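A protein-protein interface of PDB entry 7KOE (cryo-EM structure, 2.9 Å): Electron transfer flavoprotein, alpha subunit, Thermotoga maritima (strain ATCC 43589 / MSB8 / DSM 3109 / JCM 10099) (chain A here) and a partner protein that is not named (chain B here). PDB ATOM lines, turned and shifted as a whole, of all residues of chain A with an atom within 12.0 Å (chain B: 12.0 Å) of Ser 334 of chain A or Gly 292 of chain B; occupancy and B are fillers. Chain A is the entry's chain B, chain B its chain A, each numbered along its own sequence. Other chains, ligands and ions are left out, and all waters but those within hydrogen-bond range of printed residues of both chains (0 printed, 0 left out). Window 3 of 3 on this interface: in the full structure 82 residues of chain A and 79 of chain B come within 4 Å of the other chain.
O of Lys 287 of chain B lies within hydrogen-bond range of N of Gly 292 of chain B, at 3.2 Å.
The side-chain hydroxyl (OG) of Ser 334 of chain A sits close to the backbone carbonyl oxygen (O) of Gly 292 of chain B (3.4 Å).
Hydrophobic or aromatic side chains of chain B within 4 Å of the printed part of chain A: Leu 286, Pro 288 and Val 289.
Along chain B the printed residues that touch a printed residue of chain A span positions 285 to 292.
Of the 11 printed residues of chain A, 4 touch a printed residue of chain B.
Ser 334 of chain A touches just these residues of chain B: Pro 288 (3.7 Å) and Gly 292 (3.2 Å).
Gly 292 of chain B touches just one residue of chain A: Ser 334 (3.2 Å).
No residue of chain B comes within 4 Å of Lys 333 of chain A.
No residue of chain B comes within 4 Å of Gly 335 of chain A.
No residue of chain B comes within 4 Å of Val 336 of chain A.
Glu 291 of chain B touches none of the printed residues of chain A.
Of the printed residues of chain B, Leu 330 of chain A touches Pro 288 (3.6 Å) and Val 289 (3.7 Å).
Of the printed residues of chain A, Ala 285 of chain B touches Leu 331 (3.3 Å).
Printed residues of chain B within 4 Å of Leu 331 of chain A: Ala 285 (3.3 Å), Leu 286 (3.996 Å), Pro 288 (3.7 Å) and Val 289 (3.8 Å).
Printed residues of chain B within 4 Å of Leu 327 of chain A: Leu 286.
Of the printed residues of chain A, Leu 286 of chain B touches Leu 327 and Leu 331.
The nearest residue of chain B that does not touch Ser 334 of chain A is Lys 287 of chain B (5.3 Å).
The nearest printed residue of chain B that does not touch Leu 330 of chain A is Ile 271 of chain B (4.7 Å).
Leu 286 of chain B touches Leu 327 of chain A (CD2 to CD2, 3.8 Å).
O of Pro 288 of chain B touches O of Leu 330 of chain A, at 3.6 Å.
Leu 330 of chain A touches Val 289 of chain B.
Ala 285 of chain B touches Leu 331 of chain A.
Leu 331 of chain A touches Leu 286 of chain B.
Leu 331 of chain A touches Pro 288 of chain B (CD1 to CG, 3.7 Å).
Val 289 of chain B touches Leu 331 of chain A.
CB of Ser 334 of chain A touches O of Pro 288 of chain B (3.7 Å).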
ATOM      1  N   LYS A 326     -16.046 -10.464   5.279  1.00  0.00           N
ATOM      2  CA  LYS A 326     -16.657 -10.014   6.521  1.00  0.00           C
ATOM      3  C   LYS A 326     -15.695 -10.167   7.693  1.00  0.00           C
ATOM      4  O   LYS A 326     -15.753  -9.411   8.666  1.00  0.00           O
ATOM      5  CB  LYS A 326     -17.951 -10.793   6.762  1.00  0.00           C
ATOM      6  CG  LYS A 326     -18.789 -10.291   7.915  1.00  0.00           C
ATOM      7  CD  LYS A 326     -20.149 -10.944   7.916  1.00  0.00           C
ATOM      8  CE  LYS A 326     -21.037 -10.337   6.849  1.00  0.00           C
ATOM      9  NZ  LYS A 326     -21.353  -8.917   7.159  1.00  0.00           N
ATOM     10  N   LEU A 327     -14.778 -11.130   7.604  1.00  0.00           N
ATOM     11  CA  LEU A 327     -13.853 -11.357   8.708  1.00  0.00           C
ATOM     12  C   LEU A 327     -12.723 -10.335   8.712  1.00  0.00           C
ATOM     13  O   LEU A 327     -12.056 -10.147   9.735  1.00  0.00           O
ATOM     14  CB  LEU A 327     -13.299 -12.778   8.640  1.00  0.00           C
ATOM     15  CG  LEU A 327     -14.047 -13.827   9.461  1.00  0.00           C
ATOM     16  CD1 LEU A 327     -13.617 -15.219   9.065  1.00  0.00           C
ATOM     17  CD2 LEU A 327     -13.806 -13.607  10.940  1.00  0.00           C
ATOM     18  N   ARG A 328     -12.481  -9.669   7.581  1.00  0.00           N
ATOM     19  CA  ARG A 328     -11.475  -8.611   7.560  1.00  0.00           C
ATOM     20  C   ARG A 328     -11.999  -7.342   8.219  1.00  0.00           C
ATOM     21  O   ARG A 328     -11.256  -6.632   8.907  1.00  0.00           O
ATOM     22  CB  ARG A 328     -11.032  -8.323   6.123  1.00  0.00           C
ATOM     23  CG  ARG A 328     -10.062  -9.336   5.568  1.00  0.00           C
ATOM     24  CD  ARG A 328      -9.747  -9.094   4.105  1.00  0.00           C
ATOM     25  NE  ARG A 328      -9.146 -10.276   3.497  1.00  0.00           N
ATOM     26  CZ  ARG A 328      -7.846 -10.554   3.522  1.00  0.00           C
ATOM     27  NH1 ARG A 328      -7.392 -11.658   2.943  1.00  0.00           N
ATOM     28  NH2 ARG A 328      -7.001  -9.730   4.123  1.00  0.00           N
ATOM     29  N   GLU A 329     -13.284  -7.039   8.023  1.00  0.00           N
ATOM     30  CA  GLU A 329     -13.834  -5.811   8.582  1.00  0.00           C
ATOM     31  C   GLU A 329     -14.130  -5.952  10.069  1.00  0.00           C
ATOM     32  O   GLU A 329     -14.379  -4.948  10.745  1.00  0.00           O
ATOM     33  CB  GLU A 329     -15.093  -5.398   7.819  1.00  0.00           C
ATOM     34  CG  GLU A 329     -16.326  -6.211   8.143  1.00  0.00           C
ATOM     35  CD  GLU A 329     -17.352  -6.161   7.030  1.00  0.00           C
ATOM     36  OE1 GLU A 329     -16.947  -6.050   5.855  1.00  0.00           O
ATOM     37  OE2 GLU A 329     -18.562  -6.228   7.331  1.00  0.00           O
ATOM     38  N   LEU A 330     -14.108  -7.177  10.596  1.00  0.00           N
ATOM     39  CA  LEU A 330     -14.305  -7.358  12.028  1.00  0.00           C
ATOM     40  C   LEU A 330     -12.978  -7.535  12.757  1.00  0.00           C
ATOM     41  O   LEU A 330     -12.892  -7.259  13.958  1.00  0.00           O
ATOM     42  CB  LEU A 330     -15.227  -8.550  12.285  1.00  0.00           C
ATOM     43  CG  LEU A 330     -16.660  -8.496  11.739  1.00  0.00           C
ATOM     44  CD1 LEU A 330     -17.540  -9.499  12.464  1.00  0.00           C
ATOM     45  CD2 LEU A 330     -17.261  -7.100  11.825  1.00  0.00           C
ATOM     46  N   LEU A 331     -11.941  -7.986  12.057  1.00  0.00           N
ATOM     47  CA  LEU A 331     -10.601  -8.093  12.620  1.00  0.00           C
ATOM     48  C   LEU A 331      -9.867  -6.764  12.670  1.00  0.00           C
ATOM     49  O   LEU A 331      -8.875  -6.648  13.396  1.00  0.00           O
ATOM     50  CB  LEU A 331      -9.759  -9.103  11.831  1.00  0.00           C
ATOM     51  CG  LEU A 331      -9.621 -10.539  12.348  1.00  0.00           C
ATOM     52  CD1 LEU A 331      -8.752 -10.554  13.589  1.00  0.00           C
ATOM     53  CD2 LEU A 331     -10.964 -11.171  12.652  1.00  0.00           C
ATOM     54  N   ASN A 332     -10.318  -5.764  11.916  1.00  0.00           N
ATOM     55  CA  ASN A 332      -9.666  -4.463  11.926  1.00  0.00           C
ATOM     56  C   ASN A 332     -10.361  -3.472  12.852  1.00  0.00           C
ATOM     57  O   ASN A 332      -9.727  -2.506  13.288  1.00  0.00           O
ATOM     58  CB  ASN A 332      -9.603  -3.896  10.501  1.00  0.00           C
ATOM     59  CG  ASN A 332      -8.645  -2.724  10.376  1.00  0.00           C
ATOM     60  OD1 ASN A 332      -7.754  -2.543  11.206  1.00  0.00           O
ATOM     61  ND2 ASN A 332      -8.827  -1.919   9.335  1.00  0.00           N
ATOM     62  N   LYS A 333     -11.633  -3.711  13.190  1.00  0.00           N
ATOM     63  CA  LYS A 333     -12.360  -2.826  14.095  1.00  0.00           C
ATOM     64  C   LYS A 333     -11.861  -2.929  15.535  1.00  0.00           C
ATOM     65  O   LYS A 333     -12.090  -2.011  16.331  1.00  0.00           O
ATOM     66  CB  LYS A 333     -13.863  -3.125  14.024  1.00  0.00           C
ATOM     67  CG  LYS A 333     -14.408  -4.038  15.119  1.00  0.00           C
ATOM     68  CD  LYS A 333     -15.764  -4.619  14.756  1.00  0.00           C
ATOM     69  CE  LYS A 333     -16.232  -5.600  15.817  1.00  0.00           C
ATOM     70  NZ  LYS A 333     -17.116  -6.660  15.264  1.00  0.00           N
ATOM     71  N   SER A 334     -11.171  -4.019  15.886  1.00  0.00           N
ATOM     72  CA  SER A 334     -10.586  -4.196  17.209  1.00  0.00           C
ATOM     73  C   SER A 334      -9.071  -4.355  17.136  1.00  0.00           C
ATOM     74  O   SER A 334      -8.441  -4.825  18.085  1.00  0.00           O
ATOM     75  CB  SER A 334     -11.209  -5.393  17.923  1.00  0.00           C
ATOM     76  OG  SER A 334     -10.582  -5.621  19.175  1.00  0.00           O
ATOM     77  N   GLY A 335      -8.477  -3.981  16.007  1.00  0.00           N
ATOM     78  CA  GLY A 335      -7.037  -4.006  15.867  1.00  0.00           C
ATOM     79  C   GLY A 335      -6.386  -2.744  16.393  1.00  0.00           C
ATOM     80  O   GLY A 335      -5.490  -2.804  17.240  1.00  0.00           O
ATOM     81  N   VAL A 336      -6.832  -1.595  15.897  1.00  0.00           N
ATOM     82  CA  VAL A 336      -6.289  -0.312  16.323  1.00  0.00           C
ATOM     83  C   VAL A 336      -6.780   0.040  17.723  1.00  0.00           C
ATOM     84  O   VAL A 336      -5.983   0.275  18.631  1.00  0.00           O
ATOM     85  CB  VAL A 336      -6.652   0.803  15.329  1.00  0.00           C
ATOM     86  CG1 VAL A 336      -6.150   2.145  15.834  1.00  0.00           C
ATOM     87  CG2 VAL A 336      -6.083   0.495  13.955  1.00  0.00           C
ATOM     88  N   ILE B 271     -20.465 -16.777  11.612  1.00  0.00           N
ATOM     89  CA  ILE B 271     -19.843 -16.072  12.727  1.00  0.00           C
ATOM     90  C   ILE B 271     -20.836 -15.859  13.861  1.00  0.00           C
ATOM     91  O   ILE B 271     -20.423 -15.649  15.010  1.00  0.00           O
ATOM     92  CB  ILE B 271     -19.243 -14.738  12.243  1.00  0.00           C
ATOM     93  CG1 ILE B 271     -18.671 -14.902  10.840  1.00  0.00           C
ATOM     94  CG2 ILE B 271     -18.121 -14.283  13.158  1.00  0.00           C
ATOM     95  CD1 ILE B 271     -18.214 -13.610  10.208  1.00  0.00           C
ATOM     96  N   LYS B 275     -19.374 -18.146  17.753  1.00  0.00           N
ATOM     97  CA  LYS B 275     -19.233 -17.640  19.114  1.00  0.00           C
ATOM     98  C   LYS B 275     -20.050 -18.411  20.149  1.00  0.00           C
ATOM     99  O   LYS B 275     -19.895 -18.142  21.343  1.00  0.00           O
ATOM    100  CB  LYS B 275     -19.608 -16.159  19.148  1.00  0.00           C
ATOM    101  CG  LYS B 275     -18.794 -15.314  18.182  1.00  0.00           C
ATOM    102  CD  LYS B 275     -19.154 -13.842  18.276  1.00  0.00           C
ATOM    103  CE  LYS B 275     -20.492 -13.558  17.621  1.00  0.00           C
ATOM    104  NZ  LYS B 275     -20.519 -12.213  16.986  1.00  0.00           N
ATOM    105  N   VAL B 280     -13.342 -21.333  20.098  1.00  0.00           N
ATOM    106  CA  VAL B 280     -12.927 -20.175  19.306  1.00  0.00           C
ATOM    107  C   VAL B 280     -12.004 -19.250  20.087  1.00  0.00           C
ATOM    108  O   VAL B 280     -11.324 -18.405  19.490  1.00  0.00           O
ATOM    109  CB  VAL B 280     -14.201 -19.478  18.793  1.00  0.00           C
ATOM    110  CG1 VAL B 280     -13.913 -18.580  17.603  1.00  0.00           C
ATOM    111  CG2 VAL B 280     -15.212 -20.514  18.400  1.00  0.00           C
ATOM    112  N   ARG B 281     -11.927 -19.419  21.409  1.00  0.00           N
ATOM    113  CA  ARG B 281     -10.924 -18.733  22.219  1.00  0.00           C
ATOM    114  C   ARG B 281      -9.506 -19.184  21.870  1.00  0.00           C
ATOM    115  O   ARG B 281      -8.545 -18.435  22.082  1.00  0.00           O
ATOM    116  CB  ARG B 281     -11.226 -18.990  23.698  1.00  0.00           C
ATOM    117  CG  ARG B 281     -10.419 -18.182  24.701  1.00  0.00           C
ATOM    118  CD  ARG B 281     -10.680 -18.663  26.117  1.00  0.00           C
ATOM    119  NE  ARG B 281     -10.016 -19.934  26.399  1.00  0.00           N
ATOM    120  CZ  ARG B 281     -10.640 -21.107  26.452  1.00  0.00           C
ATOM    121  NH1 ARG B 281     -11.947 -21.177  26.239  1.00  0.00           N
ATOM    122  NH2 ARG B 281      -9.958 -22.212  26.713  1.00  0.00           N
ATOM    123  N   GLU B 284      -6.256 -17.931  18.347  1.00  0.00           N
ATOM    124  CA  GLU B 284      -5.215 -16.892  18.412  1.00  0.00           C
ATOM    125  C   GLU B 284      -5.356 -15.843  17.316  1.00  0.00           C
ATOM    126  O   GLU B 284      -4.459 -15.009  17.151  1.00  0.00           O
ATOM    127  CB  GLU B 284      -3.782 -17.449  18.383  1.00  0.00           C
ATOM    128  CG  GLU B 284      -3.423 -18.350  19.547  1.00  0.00           C
ATOM    129  CD  GLU B 284      -3.288 -17.598  20.850  1.00  0.00           C
ATOM    130  OE1 GLU B 284      -2.809 -16.447  20.831  1.00  0.00           O
ATOM    131  OE2 GLU B 284      -3.675 -18.158  21.894  1.00  0.00           O
ATOM    132  N   ALA B 285      -6.451 -15.864  16.557  1.00  0.00           N
ATOM    133  CA  ALA B 285      -6.726 -14.839  15.564  1.00  0.00           C
ATOM    134  C   ALA B 285      -8.198 -14.468  15.495  1.00  0.00           C
ATOM    135  O   ALA B 285      -8.575 -13.684  14.620  1.00  0.00           O
ATOM    136  CB  ALA B 285      -6.245 -15.286  14.176  1.00  0.00           C
ATOM    137  N   LEU B 286      -9.042 -15.019  16.366  1.00  0.00           N
ATOM    138  CA  LEU B 286     -10.437 -14.615  16.471  1.00  0.00           C
ATOM    139  C   LEU B 286     -10.748 -14.011  17.834  1.00  0.00           C
ATOM    140  O   LEU B 286     -11.900 -14.032  18.276  1.00  0.00           O
ATOM    141  CB  LEU B 286     -11.362 -15.794  16.175  1.00  0.00           C
ATOM    142  CG  LEU B 286     -11.462 -16.129  14.687  1.00  0.00           C
ATOM    143  CD1 LEU B 286     -12.484 -17.219  14.435  1.00  0.00           C
ATOM    144  CD2 LEU B 286     -11.788 -14.888  13.866  1.00  0.00           C
ATOM    145  N   LYS B 287      -9.736 -13.491  18.509  1.00  0.00           N
ATOM    146  CA  LYS B 287      -9.914 -12.645  19.682  1.00  0.00           C
ATOM    147  C   LYS B 287     -10.518 -11.269  19.357  1.00  0.00           C
ATOM    148  O   LYS B 287     -11.322 -10.788  20.164  1.00  0.00           O
ATOM    149  CB  LYS B 287      -8.584 -12.492  20.432  1.00  0.00           C
ATOM    150  CG  LYS B 287      -7.862 -13.799  20.708  1.00  0.00           C
ATOM    151  CD  LYS B 287      -8.261 -14.385  22.051  1.00  0.00           C
ATOM    152  CE  LYS B 287      -7.235 -15.397  22.526  1.00  0.00           C
ATOM    153  NZ  LYS B 287      -7.453 -15.796  23.943  1.00  0.00           N
ATOM    154  N   PRO B 288     -10.203 -10.587  18.237  1.00  0.00           N
ATOM    155  CA  PRO B 288     -10.945  -9.347  17.933  1.00  0.00           C
ATOM    156  C   PRO B 288     -12.413  -9.528  17.552  1.00  0.00           C
ATOM    157  O   PRO B 288     -13.086  -8.514  17.333  1.00  0.00           O
ATOM    158  CB  PRO B 288     -10.154  -8.745  16.769  1.00  0.00           C
ATOM    159  CG  PRO B 288      -8.794  -9.171  17.026  1.00  0.00           C
ATOM    160  CD  PRO B 288      -8.954 -10.595  17.439  1.00  0.00           C
ATOM    161  N   VAL B 289     -12.934 -10.749  17.442  1.00  0.00           N
ATOM    162  CA  VAL B 289     -14.371 -10.955  17.289  1.00  0.00           C
ATOM    163  C   VAL B 289     -14.983 -11.655  18.489  1.00  0.00           C
ATOM    164  O   VAL B 289     -16.212 -11.808  18.542  1.00  0.00           O
ATOM    165  CB  VAL B 289     -14.709 -11.722  15.995  1.00  0.00           C
ATOM    166  CG1 VAL B 289     -14.068 -11.056  14.794  1.00  0.00           C
ATOM    167  CG2 VAL B 289     -14.276 -13.166  16.100  1.00  0.00           C
ATOM    168  N   LEU B 290     -14.171 -12.087  19.452  1.00  0.00           N
ATOM    169  CA  LEU B 290     -14.655 -12.675  20.694  1.00  0.00           C
ATOM    170  C   LEU B 290     -14.411 -11.778  21.897  1.00  0.00           C
ATOM    171  O   LEU B 290     -15.346 -11.477  22.645  1.00  0.00           O
ATOM    172  CB  LEU B 290     -14.003 -14.047  20.931  1.00  0.00           C
ATOM    173  CG  LEU B 290     -14.774 -15.303  20.514  1.00  0.00           C
ATOM    174  CD1 LEU B 290     -16.037 -15.448  21.347  1.00  0.00           C
ATOM    175  CD2 LEU B 290     -15.108 -15.308  19.035  1.00  0.00           C
ATOM    176  N   GLU B 291     -13.167 -11.344  22.107  1.00  0.00           N
ATOM    177  CA  GLU B 291     -12.884 -10.395  23.178  1.00  0.00           C
ATOM    178  C   GLU B 291     -13.421  -9.010  22.834  1.00  0.00           C
ATOM    179  O   GLU B 291     -14.171  -8.412  23.614  1.00  0.00           O
ATOM    180  CB  GLU B 291     -11.378 -10.340  23.447  1.00  0.00           C
ATOM    181  CG  GLU B 291     -10.964  -9.372  24.547  1.00  0.00           C
ATOM    182  CD  GLU B 291     -11.418  -9.804  25.928  1.00  0.00           C
ATOM    183  OE1 GLU B 291     -11.572 -11.021  26.161  1.00  0.00           O
ATOM    184  OE2 GLU B 291     -11.621  -8.921  26.786  1.00  0.00           O
ATOM    185  N   GLY B 292     -13.057  -8.492  21.666  1.00  0.00           N
ATOM    186  CA  GLY B 292     -13.516  -7.188  21.228  1.00  0.00           C
ATOM    187  C   GLY B 292     -12.573  -6.066  21.613  1.00  0.00           C
ATOM    188  O   GLY B 292     -11.594  -6.284  22.328  1.00  0.00           O
